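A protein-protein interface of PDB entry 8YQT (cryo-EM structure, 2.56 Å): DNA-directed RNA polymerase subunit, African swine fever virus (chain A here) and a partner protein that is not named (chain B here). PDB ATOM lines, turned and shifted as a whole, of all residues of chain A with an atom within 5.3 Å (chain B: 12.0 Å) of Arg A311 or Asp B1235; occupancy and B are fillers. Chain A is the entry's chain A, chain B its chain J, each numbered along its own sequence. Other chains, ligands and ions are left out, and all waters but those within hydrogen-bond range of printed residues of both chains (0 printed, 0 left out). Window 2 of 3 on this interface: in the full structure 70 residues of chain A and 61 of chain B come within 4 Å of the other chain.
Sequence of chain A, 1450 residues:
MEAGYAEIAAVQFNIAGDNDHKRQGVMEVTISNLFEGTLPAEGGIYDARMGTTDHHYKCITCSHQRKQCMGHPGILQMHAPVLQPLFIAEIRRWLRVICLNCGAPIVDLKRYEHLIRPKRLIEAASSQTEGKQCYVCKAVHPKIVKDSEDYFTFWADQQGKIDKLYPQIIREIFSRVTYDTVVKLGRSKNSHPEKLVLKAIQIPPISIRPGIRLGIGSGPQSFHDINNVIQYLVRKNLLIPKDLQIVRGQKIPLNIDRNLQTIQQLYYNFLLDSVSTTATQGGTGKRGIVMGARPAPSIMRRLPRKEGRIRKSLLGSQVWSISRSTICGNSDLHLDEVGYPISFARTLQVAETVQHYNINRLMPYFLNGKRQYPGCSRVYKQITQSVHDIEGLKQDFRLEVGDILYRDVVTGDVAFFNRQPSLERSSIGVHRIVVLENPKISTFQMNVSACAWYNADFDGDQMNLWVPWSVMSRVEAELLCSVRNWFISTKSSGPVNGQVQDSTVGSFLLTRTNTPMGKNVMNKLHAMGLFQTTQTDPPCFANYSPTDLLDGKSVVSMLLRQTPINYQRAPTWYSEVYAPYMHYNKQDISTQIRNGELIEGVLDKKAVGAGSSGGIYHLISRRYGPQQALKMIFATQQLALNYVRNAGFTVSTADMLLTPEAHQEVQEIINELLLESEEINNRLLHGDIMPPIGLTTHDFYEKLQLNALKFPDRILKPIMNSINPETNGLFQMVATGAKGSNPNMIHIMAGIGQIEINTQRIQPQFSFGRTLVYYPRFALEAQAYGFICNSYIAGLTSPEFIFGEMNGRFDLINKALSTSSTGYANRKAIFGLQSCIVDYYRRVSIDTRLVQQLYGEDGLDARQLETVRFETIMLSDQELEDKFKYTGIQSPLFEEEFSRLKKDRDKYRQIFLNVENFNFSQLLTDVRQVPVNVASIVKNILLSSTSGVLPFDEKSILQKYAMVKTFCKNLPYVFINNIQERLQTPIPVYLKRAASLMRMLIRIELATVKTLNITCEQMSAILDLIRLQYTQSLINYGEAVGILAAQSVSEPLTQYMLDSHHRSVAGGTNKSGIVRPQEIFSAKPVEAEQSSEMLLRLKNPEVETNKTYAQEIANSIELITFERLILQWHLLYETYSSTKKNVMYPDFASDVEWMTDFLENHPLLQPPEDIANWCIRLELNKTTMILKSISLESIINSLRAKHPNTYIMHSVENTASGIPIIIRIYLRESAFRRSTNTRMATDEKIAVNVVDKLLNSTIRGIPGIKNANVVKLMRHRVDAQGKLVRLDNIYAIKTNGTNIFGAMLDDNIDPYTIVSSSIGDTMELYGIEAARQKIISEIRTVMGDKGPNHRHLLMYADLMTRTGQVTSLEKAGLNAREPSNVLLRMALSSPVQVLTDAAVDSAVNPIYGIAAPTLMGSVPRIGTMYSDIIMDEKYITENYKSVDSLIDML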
ATOM      1  N   LEU A 303     -20.111 -13.582 -33.243  1.00  0.00           N
ATOM      2  CA  LEU A 303     -20.800 -12.311 -33.047  1.00  0.00           C
ATOM      3  C   LEU A 303     -20.161 -11.351 -32.041  1.00  0.00           C
ATOM      4  O   LEU A 303     -19.905 -10.192 -32.387  1.00  0.00           O
ATOM      5  CB  LEU A 303     -22.245 -12.592 -32.627  1.00  0.00           C
ATOM      6  CG  LEU A 303     -23.306 -12.695 -33.722  1.00  0.00           C
ATOM      7  CD1 LEU A 303     -22.994 -13.820 -34.687  1.00  0.00           C
ATOM      8  CD2 LEU A 303     -24.669 -12.906 -33.098  1.00  0.00           C
ATOM      9  N   PRO A 304     -19.886 -11.782 -30.788  1.00  0.00           N
ATOM     10  CA  PRO A 304     -19.891 -10.832 -29.661  1.00  0.00           C
ATOM     11  C   PRO A 304     -18.853  -9.716 -29.651  1.00  0.00           C
ATOM     12  O   PRO A 304     -19.221  -8.544 -29.537  1.00  0.00           O
ATOM     13  CB  PRO A 304     -19.682 -11.748 -28.446  1.00  0.00           C
ATOM     14  CG  PRO A 304     -20.039 -13.110 -28.920  1.00  0.00           C
ATOM     15  CD  PRO A 304     -19.568 -13.140 -30.322  1.00  0.00           C
ATOM     16  N   ARG A 305     -17.570 -10.044 -29.747  1.00  0.00           N
ATOM     17  CA  ARG A 305     -16.541  -9.129 -29.273  1.00  0.00           C
ATOM     18  C   ARG A 305     -16.128  -8.128 -30.351  1.00  0.00           C
ATOM     19  O   ARG A 305     -16.753  -8.011 -31.409  1.00  0.00           O
ATOM     20  CB  ARG A 305     -15.337  -9.914 -28.762  1.00  0.00           C
ATOM     21  CG  ARG A 305     -15.413 -10.266 -27.291  1.00  0.00           C
ATOM     22  CD  ARG A 305     -14.796 -11.629 -27.028  1.00  0.00           C
ATOM     23  NE  ARG A 305     -15.698 -12.716 -27.385  1.00  0.00           N
ATOM     24  CZ  ARG A 305     -16.703 -13.135 -26.629  1.00  0.00           C
ATOM     25  NH1 ARG A 305     -16.963 -12.582 -25.456  1.00  0.00           N
ATOM     26  NH2 ARG A 305     -17.466 -14.135 -27.059  1.00  0.00           N
ATOM     27  N   LYS A 306     -15.055  -7.385 -30.068  1.00  0.00           N
ATOM     28  CA  LYS A 306     -14.541  -6.384 -30.994  1.00  0.00           C
ATOM     29  C   LYS A 306     -14.009  -7.017 -32.271  1.00  0.00           C
ATOM     30  O   LYS A 306     -14.060  -6.398 -33.339  1.00  0.00           O
ATOM     31  CB  LYS A 306     -13.452  -5.567 -30.300  1.00  0.00           C
ATOM     32  CG  LYS A 306     -12.770  -4.529 -31.162  1.00  0.00           C
ATOM     33  CD  LYS A 306     -11.325  -4.906 -31.421  1.00  0.00           C
ATOM     34  CE  LYS A 306     -10.509  -3.686 -31.798  1.00  0.00           C
ATOM     35  NZ  LYS A 306     -10.424  -2.732 -30.659  1.00  0.00           N
ATOM     36  N   GLY A 308     -15.416  -9.634 -33.477  1.00  0.00           N
ATOM     37  CA  GLY A 308     -16.546 -10.423 -33.917  1.00  0.00           C
ATOM     38  C   GLY A 308     -17.191  -9.892 -35.179  1.00  0.00           C
ATOM     39  O   GLY A 308     -16.700  -8.966 -35.827  1.00  0.00           O
ATOM     40  N   ARG A 309     -18.323 -10.503 -35.529  1.00  0.00           N
ATOM     41  CA  ARG A 309     -19.013 -10.161 -36.768  1.00  0.00           C
ATOM     42  C   ARG A 309     -19.500  -8.717 -36.758  1.00  0.00           C
ATOM     43  O   ARG A 309     -19.259  -7.964 -37.706  1.00  0.00           O
ATOM     44  CB  ARG A 309     -20.191 -11.113 -36.984  1.00  0.00           C
ATOM     45  CG  ARG A 309     -20.975 -10.860 -38.262  1.00  0.00           C
ATOM     46  CD  ARG A 309     -20.136 -11.218 -39.463  1.00  0.00           C
ATOM     47  NE  ARG A 309     -19.744 -12.620 -39.414  1.00  0.00           N
ATOM     48  CZ  ARG A 309     -18.566 -13.082 -39.804  1.00  0.00           C
ATOM     49  NH1 ARG A 309     -17.625 -12.275 -40.260  1.00  0.00           N
ATOM     50  NH2 ARG A 309     -18.321 -14.387 -39.720  1.00  0.00           N
ATOM     51  N   ILE A 310     -20.187  -8.315 -35.690  1.00  0.00           N
ATOM     52  CA  ILE A 310     -20.898  -7.041 -35.697  1.00  0.00           C
ATOM     53  C   ILE A 310     -19.929  -5.869 -35.715  1.00  0.00           C
ATOM     54  O   ILE A 310     -20.104  -4.915 -36.480  1.00  0.00           O
ATOM     55  CB  ILE A 310     -21.858  -6.973 -34.497  1.00  0.00           C
ATOM     56  CG1 ILE A 310     -22.954  -8.024 -34.653  1.00  0.00           C
ATOM     57  CG2 ILE A 310     -22.448  -5.584 -34.357  1.00  0.00           C
ATOM     58  CD1 ILE A 310     -23.803  -8.193 -33.440  1.00  0.00           C
ATOM     59  N   ARG A 311     -18.891  -5.913 -34.882  1.00  0.00           N
ATOM     60  CA  ARG A 311     -18.022  -4.752 -34.749  1.00  0.00           C
ATOM     61  C   ARG A 311     -16.930  -4.727 -35.810  1.00  0.00           C
ATOM     62  O   ARG A 311     -16.543  -3.650 -36.275  1.00  0.00           O
ATOM     63  CB  ARG A 311     -17.414  -4.711 -33.348  1.00  0.00           C
ATOM     64  CG  ARG A 311     -18.409  -4.295 -32.284  1.00  0.00           C
ATOM     65  CD  ARG A 311     -17.810  -4.348 -30.899  1.00  0.00           C
ATOM     66  NE  ARG A 311     -16.639  -3.490 -30.789  1.00  0.00           N
ATOM     67  CZ  ARG A 311     -15.993  -3.247 -29.658  1.00  0.00           C
ATOM     68  NH1 ARG A 311     -16.388  -3.771 -28.510  1.00  0.00           N
ATOM     69  NH2 ARG A 311     -14.929  -2.450 -29.679  1.00  0.00           N
ATOM     70  N   LYS A 312     -16.419  -5.891 -36.209  1.00  0.00           N
ATOM     71  CA  LYS A 312     -15.313  -5.907 -37.157  1.00  0.00           C
ATOM     72  C   LYS A 312     -15.794  -5.872 -38.603  1.00  0.00           C
ATOM     73  O   LYS A 312     -15.131  -5.284 -39.462  1.00  0.00           O
ATOM     74  CB  LYS A 312     -14.436  -7.132 -36.924  1.00  0.00           C
ATOM     75  CG  LYS A 312     -13.051  -7.005 -37.514  1.00  0.00           C
ATOM     76  CD  LYS A 312     -12.569  -8.323 -38.077  1.00  0.00           C
ATOM     77  CE  LYS A 312     -11.186  -8.181 -38.679  1.00  0.00           C
ATOM     78  NZ  LYS A 312     -10.726  -9.442 -39.320  1.00  0.00           N
ATOM     79  N   SER A 313     -16.934  -6.490 -38.895  1.00  0.00           N
ATOM     80  CA  SER A 313     -17.407  -6.610 -40.269  1.00  0.00           C
ATOM     81  C   SER A 313     -18.534  -5.648 -40.607  1.00  0.00           C
ATOM     82  O   SER A 313     -18.577  -5.129 -41.724  1.00  0.00           O
ATOM     83  CB  SER A 313     -17.866  -8.043 -40.546  1.00  0.00           C
ATOM     84  OG  SER A 313     -16.787  -8.951 -40.438  1.00  0.00           O
ATOM     85  N   LEU A 314     -19.443  -5.390 -39.673  1.00  0.00           N
ATOM     86  CA  LEU A 314     -20.626  -4.584 -39.949  1.00  0.00           C
ATOM     87  C   LEU A 314     -20.452  -3.117 -39.593  1.00  0.00           C
ATOM     88  O   LEU A 314     -20.792  -2.247 -40.398  1.00  0.00           O
ATOM     89  CB  LEU A 314     -21.832  -5.147 -39.196  1.00  0.00           C
ATOM     90  CG  LEU A 314     -22.243  -6.551 -39.630  1.00  0.00           C
ATOM     91  CD1 LEU A 314     -23.334  -7.094 -38.737  1.00  0.00           C
ATOM     92  CD2 LEU A 314     -22.690  -6.508 -41.067  1.00  0.00           C
ATOM     93  N   LEU A 315     -19.937  -2.820 -38.404  1.00  0.00           N
ATOM     94  CA  LEU A 315     -19.740  -1.444 -37.977  1.00  0.00           C
ATOM     95  C   LEU A 315     -18.438  -0.847 -38.493  1.00  0.00           C
ATOM     96  O   LEU A 315     -18.258   0.371 -38.412  1.00  0.00           O
ATOM     97  CB  LEU A 315     -19.784  -1.363 -36.450  1.00  0.00           C
ATOM     98  CG  LEU A 315     -21.092  -1.848 -35.824  1.00  0.00           C
ATOM     99  CD1 LEU A 315     -20.994  -1.873 -34.312  1.00  0.00           C
ATOM    100  CD2 LEU A 315     -22.253  -0.987 -36.272  1.00  0.00           C
ATOM    101  N   GLY A 316     -17.538  -1.675 -39.021  1.00  0.00           N
ATOM    102  CA  GLY A 316     -16.336  -1.207 -39.675  1.00  0.00           C
ATOM    103  C   GLY A 316     -16.148  -1.944 -40.985  1.00  0.00           C
ATOM    104  O   GLY A 316     -16.959  -2.791 -41.355  1.00  0.00           O
ATOM    105  N   GLY A 823     -12.194   5.452 -24.452  1.00  0.00           N
ATOM    106  CA  GLY A 823     -12.881   4.655 -25.453  1.00  0.00           C
ATOM    107  C   GLY A 823     -14.093   3.929 -24.901  1.00  0.00           C
ATOM    108  O   GLY A 823     -15.095   3.760 -25.598  1.00  0.00           O
ATOM    109  N   TYR A 824     -14.013   3.475 -23.649  1.00  0.00           N
ATOM    110  CA  TYR A 824     -15.158   2.825 -23.022  1.00  0.00           C
ATOM    111  C   TYR A 824     -16.314   3.801 -22.845  1.00  0.00           C
ATOM    112  O   TYR A 824     -17.474   3.457 -23.088  1.00  0.00           O
ATOM    113  CB  TYR A 824     -14.749   2.227 -21.677  1.00  0.00           C
ATOM    114  CG  TYR A 824     -13.882   0.995 -21.780  1.00  0.00           C
ATOM    115  CD1 TYR A 824     -14.275  -0.089 -22.549  1.00  0.00           C
ATOM    116  CD2 TYR A 824     -12.675   0.913 -21.100  1.00  0.00           C
ATOM    117  CE1 TYR A 824     -13.490  -1.220 -22.644  1.00  0.00           C
ATOM    118  CE2 TYR A 824     -11.883  -0.214 -21.189  1.00  0.00           C
ATOM    119  CZ  TYR A 824     -12.296  -1.276 -21.964  1.00  0.00           C
ATOM    120  OH  TYR A 824     -11.510  -2.400 -22.054  1.00  0.00           O
ATOM    121  N   ARG A 827     -17.763   4.993 -26.526  1.00  0.00           N
ATOM    122  CA  ARG A 827     -18.612   4.059 -27.257  1.00  0.00           C
ATOM    123  C   ARG A 827     -19.984   3.914 -26.614  1.00  0.00           C
ATOM    124  O   ARG A 827     -20.974   3.710 -27.321  1.00  0.00           O
ATOM    125  CB  ARG A 827     -17.926   2.699 -27.364  1.00  0.00           C
ATOM    126  CG  ARG A 827     -18.604   1.774 -28.341  1.00  0.00           C
ATOM    127  CD  ARG A 827     -17.790   0.538 -28.634  1.00  0.00           C
ATOM    128  NE  ARG A 827     -18.406  -0.241 -29.701  1.00  0.00           N
ATOM    129  CZ  ARG A 827     -19.405  -1.094 -29.527  1.00  0.00           C
ATOM    130  NH1 ARG A 827     -19.917  -1.326 -28.333  1.00  0.00           N
ATOM    131  NH2 ARG A 827     -19.906  -1.727 -30.583  1.00  0.00           N
ATOM    132  N   ALA A1387     -25.610  -4.451 -31.219  1.00  0.00           N
ATOM    133  CA  ALA A1387     -24.314  -3.889 -31.579  1.00  0.00           C
ATOM    134  C   ALA A1387     -23.555  -3.385 -30.360  1.00  0.00           C
ATOM    135  O   ALA A1387     -22.322  -3.436 -30.339  1.00  0.00           O
ATOM    136  CB  ALA A1387     -24.497  -2.765 -32.597  1.00  0.00           C
ATOM    137  N   LEU B1227     -14.774  -5.789 -14.539  1.00  0.00           N
ATOM    138  CA  LEU B1227     -14.105  -6.925 -15.164  1.00  0.00           C
ATOM    139  C   LEU B1227     -13.383  -6.503 -16.440  1.00  0.00           C
ATOM    140  O   LEU B1227     -12.599  -7.266 -17.002  1.00  0.00           O
ATOM    141  CB  LEU B1227     -15.108  -8.038 -15.469  1.00  0.00           C
ATOM    142  CG  LEU B1227     -15.187  -9.178 -14.451  1.00  0.00           C
ATOM    143  CD1 LEU B1227     -13.856  -9.914 -14.374  1.00  0.00           C
ATOM    144  CD2 LEU B1227     -15.604  -8.667 -13.080  1.00  0.00           C
ATOM    145  N   ASP B1228     -13.658  -5.284 -16.894  1.00  0.00           N
ATOM    146  CA  ASP B1228     -12.960  -4.745 -18.052  1.00  0.00           C
ATOM    147  C   ASP B1228     -11.523  -4.403 -17.684  1.00  0.00           C
ATOM    148  O   ASP B1228     -11.246  -3.905 -16.590  1.00  0.00           O
ATOM    149  CB  ASP B1228     -13.674  -3.499 -18.575  1.00  0.00           C
ATOM    150  CG  ASP B1228     -15.033  -3.809 -19.171  1.00  0.00           C
ATOM    151  OD1 ASP B1228     -15.226  -4.946 -19.652  1.00  0.00           O
ATOM    152  OD2 ASP B1228     -15.906  -2.916 -19.160  1.00  0.00           O
ATOM    153  N   ASP B1229     -10.608  -4.675 -18.601  1.00  0.00           N
ATOM    154  CA  ASP B1229      -9.217  -4.297 -18.393  1.00  0.00           C
ATOM    155  C   ASP B1229      -9.085  -2.790 -18.557  1.00  0.00           C
ATOM    156  O   ASP B1229      -9.405  -2.264 -19.631  1.00  0.00           O
ATOM    157  CB  ASP B1229      -8.314  -5.028 -19.379  1.00  0.00           C
ATOM    158  CG  ASP B1229      -6.870  -5.071 -18.928  1.00  0.00           C
ATOM    159  OD1 ASP B1229      -6.340  -4.025 -18.500  1.00  0.00           O
ATOM    160  OD2 ASP B1229      -6.264  -6.158 -19.000  1.00  0.00           O
ATOM    161  N   PRO B1230      -8.632  -2.059 -17.535  1.00  0.00           N
ATOM    162  CA  PRO B1230      -8.554  -0.596 -17.659  1.00  0.00           C
ATOM    163  C   PRO B1230      -7.570  -0.113 -18.709  1.00  0.00           C
ATOM    164  O   PRO B1230      -7.723   1.012 -19.197  1.00  0.00           O
ATOM    165  CB  PRO B1230      -8.137  -0.145 -16.253  1.00  0.00           C
ATOM    166  CG  PRO B1230      -7.506  -1.339 -15.639  1.00  0.00           C
ATOM    167  CD  PRO B1230      -8.223  -2.525 -16.201  1.00  0.00           C
ATOM    168  N   PHE B1231      -6.571  -0.915 -19.077  1.00  0.00           N
ATOM    169  CA  PHE B1231      -5.546  -0.490 -20.019  1.00  0.00           C
ATOM    170  C   PHE B1231      -5.712  -1.093 -21.405  1.00  0.00           C
ATOM    171  O   PHE B1231      -4.944  -0.749 -22.308  1.00  0.00           O
ATOM    172  CB  PHE B1231      -4.149  -0.828 -19.483  1.00  0.00           C
ATOM    173  CG  PHE B1231      -3.734   0.001 -18.303  1.00  0.00           C
ATOM    174  CD1 PHE B1231      -4.297  -0.212 -17.055  1.00  0.00           C
ATOM    175  CD2 PHE B1231      -2.806   1.015 -18.449  1.00  0.00           C
ATOM    176  CE1 PHE B1231      -3.923   0.554 -15.974  1.00  0.00           C
ATOM    177  CE2 PHE B1231      -2.431   1.785 -17.370  1.00  0.00           C
ATOM    178  CZ  PHE B1231      -2.989   1.554 -16.131  1.00  0.00           C
ATOM    179  N   SER B1232      -6.684  -1.977 -21.601  1.00  0.00           N
ATOM    180  CA  SER B1232      -6.897  -2.582 -22.907  1.00  0.00           C
ATOM    181  C   SER B1232      -7.671  -1.635 -23.811  1.00  0.00           C
ATOM    182  O   SER B1232      -8.661  -1.027 -23.394  1.00  0.00           O
ATOM    183  CB  SER B1232      -7.654  -3.901 -22.771  1.00  0.00           C
ATOM    184  OG  SER B1232      -9.002  -3.673 -22.397  1.00  0.00           O
ATOM    185  N   ILE B1233      -7.215  -1.509 -25.051  1.00  0.00           N
ATOM    186  CA  ILE B1233      -7.947  -0.731 -26.061  1.00  0.00           C
ATOM    187  C   ILE B1233      -8.908  -1.712 -26.724  1.00  0.00           C
ATOM    188  O   ILE B1233      -8.657  -2.276 -27.791  1.00  0.00           O
ATOM    189  CB  ILE B1233      -7.009  -0.040 -27.054  1.00  0.00           C
ATOM    190  CG1 ILE B1233      -5.893  -0.988 -27.495  1.00  0.00           C
ATOM    191  CG2 ILE B1233      -6.417   1.214 -26.437  1.00  0.00           C
ATOM    192  CD1 ILE B1233      -5.133  -0.505 -28.699  1.00  0.00           C
ATOM    193  N   GLU B1234     -10.048  -1.916 -26.069  1.00  0.00           N
ATOM    194  CA  GLU B1234     -11.088  -2.820 -26.541  1.00  0.00           C
ATOM    195  C   GLU B1234     -12.206  -2.093 -27.269  1.00  0.00           C
ATOM    196  O   GLU B1234     -12.689  -2.578 -28.297  1.00  0.00           O
ATOM    197  CB  GLU B1234     -11.666  -3.611 -25.363  1.00  0.00           C
ATOM    198  CG  GLU B1234     -12.851  -4.500 -25.701  1.00  0.00           C
ATOM    199  CD  GLU B1234     -12.466  -5.710 -26.528  1.00  0.00           C
ATOM    200  OE1 GLU B1234     -11.260  -6.031 -26.588  1.00  0.00           O
ATOM    201  OE2 GLU B1234     -13.370  -6.349 -27.105  1.00  0.00           O
ATOM    202  N   ASP B1235     -12.624  -0.934 -26.762  1.00  0.00           N
ATOM    203  CA  ASP B1235     -13.631  -0.109 -27.410  1.00  0.00           C
ATOM    204  C   ASP B1235     -13.012   0.992 -28.259  1.00  0.00           C
ATOM    205  O   ASP B1235     -13.724   1.897 -28.709  1.00  0.00           O
ATOM    206  CB  ASP B1235     -14.579   0.488 -26.370  1.00  0.00           C
ATOM    207  CG  ASP B1235     -15.544  -0.536 -25.806  1.00  0.00           C
ATOM    208  OD1 ASP B1235     -15.562  -1.679 -26.304  1.00  0.00           O
ATOM    209  OD2 ASP B1235     -16.303  -0.192 -24.877  1.00  0.00           O
ATOM    210  N   VAL B1236     -11.704   0.938 -28.482  1.00  0.00           N
ATOM    211  CA  VAL B1236     -11.003   1.882 -29.341  1.00  0.00           C
ATOM    212  C   VAL B1236     -10.694   1.162 -30.645  1.00  0.00           C
ATOM    213  O   VAL B1236      -9.913   0.202 -30.668  1.00  0.00           O
ATOM    214  CB  VAL B1236      -9.723   2.417 -28.685  1.00  0.00           C
ATOM    215  CG1 VAL B1236      -9.008   3.375 -29.626  1.00  0.00           C
ATOM    216  CG2 VAL B1236     -10.053   3.096 -27.372  1.00  0.00           C
ATOM    217  N   ASP B1237     -11.308   1.623 -31.733  1.00  0.00           N
ATOM    218  CA  ASP B1237     -11.140   1.003 -33.046  1.00  0.00           C
ATOM    219  C   ASP B1237      -9.987   1.700 -33.763  1.00  0.00           C
ATOM    220  O   ASP B1237     -10.168   2.555 -34.631  1.00  0.00           O
ATOM    221  CB  ASP B1237     -12.440   1.076 -33.838  1.00  0.00           C
ATOM    222  CG  ASP B1237     -12.490   0.075 -34.970  1.00  0.00           C
ATOM    223  OD1 ASP B1237     -11.445  -0.528 -35.284  1.00  0.00           O
ATOM    224  OD2 ASP B1237     -13.582  -0.117 -35.541  1.00  0.00           O
ATOM    225  N   ILE B1238      -8.773   1.316 -33.382  1.00  0.00           N
ATOM    226  CA  ILE B1238      -7.553   1.871 -33.948  1.00  0.00           C
ATOM    227  C   ILE B1238      -6.695   0.727 -34.467  1.00  0.00           C
ATOM    228  O   ILE B1238      -6.656  -0.363 -33.887  1.00  0.00           O
ATOM    229  CB  ILE B1238      -6.779   2.730 -32.920  1.00  0.00           C
ATOM    230  CG1 ILE B1238      -5.669   3.525 -33.605  1.00  0.00           C
ATOM    231  CG2 ILE B1238      -6.215   1.872 -31.794  1.00  0.00           C
ATOM    232  CD1 ILE B1238      -5.014   4.536 -32.710  1.00  0.00           C
ATOM    233  N   SER B1239      -6.026   0.973 -35.587  1.00  0.00           N
ATOM    234  CA  SER B1239      -5.172  -0.039 -36.188  1.00  0.00           C
ATOM    235  C   SER B1239      -3.952  -0.302 -35.314  1.00  0.00           C
ATOM    236  O   SER B1239      -3.469   0.579 -34.599  1.00  0.00           O
ATOM    237  CB  SER B1239      -4.732   0.395 -37.585  1.00  0.00           C
ATOM    238  OG  SER B1239      -3.812  -0.528 -38.136  1.00  0.00           O
ATOM    239  N   LEU B1240      -3.453  -1.537 -35.378  1.00  0.00           N
ATOM    240  CA  LEU B1240      -2.287  -1.917 -34.590  1.00  0.00           C
ATOM    241  C   LEU B1240      -0.983  -1.422 -35.196  1.00  0.00           C
ATOM    242  O   LEU B1240       0.047  -1.438 -34.514  1.00  0.00           O
ATOM    243  CB  LEU B1240      -2.235  -3.436 -34.423  1.00  0.00           C
ATOM    244  CG  LEU B1240      -3.436  -4.075 -33.722  1.00  0.00           C
ATOM    245  CD1 LEU B1240      -3.241  -5.575 -33.590  1.00  0.00           C
ATOM    246  CD2 LEU B1240      -3.682  -3.437 -32.362  1.00  0.00           C
ATOM    247  N   LEU B1243      -0.511   2.514 -33.703  1.00  0.00           N
ATOM    248  CA  LEU B1243      -0.466   2.715 -32.256  1.00  0.00           C
ATOM    249  C   LEU B1243       0.560   3.750 -31.806  1.00  0.00           C
ATOM    250  O   LEU B1243       0.485   4.203 -30.660  1.00  0.00           O
ATOM    251  CB  LEU B1243      -0.182   1.387 -31.554  1.00  0.00           C
ATOM    252  CG  LEU B1243      -1.287   0.334 -31.612  1.00  0.00           C
ATOM    253  CD1 LEU B1243      -0.858  -0.925 -30.883  1.00  0.00           C
ATOM    254  CD2 LEU B1243      -2.575   0.881 -31.029  1.00  0.00           C
ATOM    255  N   LEU B1246      -0.631   7.134 -30.398  1.00  0.00           N
ATOM    256  CA  LEU B1246      -0.963   7.250 -28.987  1.00  0.00           C
ATOM    257  C   LEU B1246       0.243   7.592 -28.123  1.00  0.00           C
ATOM    258  O   LEU B1246       0.111   7.662 -26.899  1.00  0.00           O
ATOM    259  CB  LEU B1246      -1.604   5.950 -28.494  1.00  0.00           C
ATOM    260  CG  LEU B1246      -2.897   5.528 -29.192  1.00  0.00           C
ATOM    261  CD1 LEU B1246      -3.379   4.192 -28.663  1.00  0.00           C
ATOM    262  CD2 LEU B1246      -3.966   6.590 -29.026  1.00  0.00           C
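Pro A304 touches none of the printed residues of chain B. No residue of chain B comes within 4 Å of Ile A310. Arg A311 touches two residues of chain B. No residue of chain B comes within 4 Å of Leu A314. No residue of chain B comes within 4 Å of Leu A315. No residue of chain B comes within 4 Å of Gly A316. Of chain B, only Asp B1235 (3.4 Å) and Val B1236 (3.8 Å) come within 4 Å of Gly A823. Of chain B, only Asp B1229, Ser B1232, Glu B1234 and Asp B1235 come within 4 Å of Tyr A824. Arg A827 touches just one residue of chain B: Asp B1235. Of the printed residues of chain A, Asp B1229 touches Tyr A824. Printed residues of chain A within 4 Å of Ser B1232: Tyr A824 (2.8 Å). Of the printed residues of chain A, Ile B1233 touches Lys A306 (3.4 Å). Of the printed residues of chain A, Glu B1234 touches Lys A306, Arg A311 and Tyr A824. Of chain A, only Arg A311 (3.2 Å), Gly A823 (3.4 Å), Tyr A824 (3.1 Å) and Arg A827 (3.8 Å) come within 4 Å of Asp B1235. Printed residues of chain A within 4 Å of Val B1236: Lys A306 (3.0 Å) and Gly A823 (3.8 Å). Ile B1238 touches none of the printed residues of chain A. The nearest printed residue of chain A that does not touch Asp B1229 is Gly A823 (9.4 Å).
Among the printed residues, merely in contact across the chains: Gly A823 with Asp B1235 (3.4 Å), Gly A823 with Val B1236 (3.8 Å), Tyr A824 with Glu B1234 (3.5 Å), Tyr A824 with Asp B1235 (3.1 Å) and Arg A827 with Asp B1235 (3.8 Å).
O of Ile B1233 lies within hydrogen-bond range of NZ of Lys A306 (3.4 Å). NZ of Lys A306 is in hydrogen-bond range of O of Glu B1234 (3.3 Å). The side-chain amino group (NZ) of Lys A306 is in hydrogen-bond range of the backbone carbonyl oxygen (O) of Val B1236, 3.0 Å away. The backbone carbonyl oxygen of Glu B1234 is in hydrogen-bond range of the guanidinium group of Arg A311. The side-chain carboxylate of Asp B1235 is in salt-bridge range of the guanidinium group of Arg A311, 3.2 Å away. The backbone carbonyl oxygen of Asp B1229 sits at hydrogen-bond distance from the side-chain hydroxyl of Tyr A824, 3.2 Å away. The side-chain hydroxyl (OH) of Tyr A824 is in hydrogen-bond range of the side-chain hydroxyl (OG) of Ser B1232 (2.8 Å).
The backbone carbonyl oxygen of Ala A1387 sits at hydrogen-bond distance from the guanidinium group of Arg A827 (3.0 Å). OD1 of Asp B1229 sits at hydrogen-bond distance from N of Phe B1231, 3.2 Å away. The side-chain hydroxyl (OG) of Ser B1232 lies within hydrogen-bond range of the backbone carbonyl oxygen (O) of Asp B1229 (3.1 Å).
Printed residues of chain A that touch a printed residue of chain B: Lys A306, Arg A311, Gly A823, Tyr A824 and Arg A827. Hydrophobic or aromatic side chains of chain A within 4 Å of the printed part of chain B: Tyr A824. Of the 16 printed residues of chain B, 6 touch a printed residue of chain A. Hydrophobic or aromatic side chains of chain B that line the printed part of chain A: Val B1236. Among the printed residues, 12 pairs touch across the chains. Among the printed residues, Asp or Glu carboxylates within 4 Å of a Lys or Arg side-chain nitrogen of the other chain: Arg A311 with Asp B1235.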
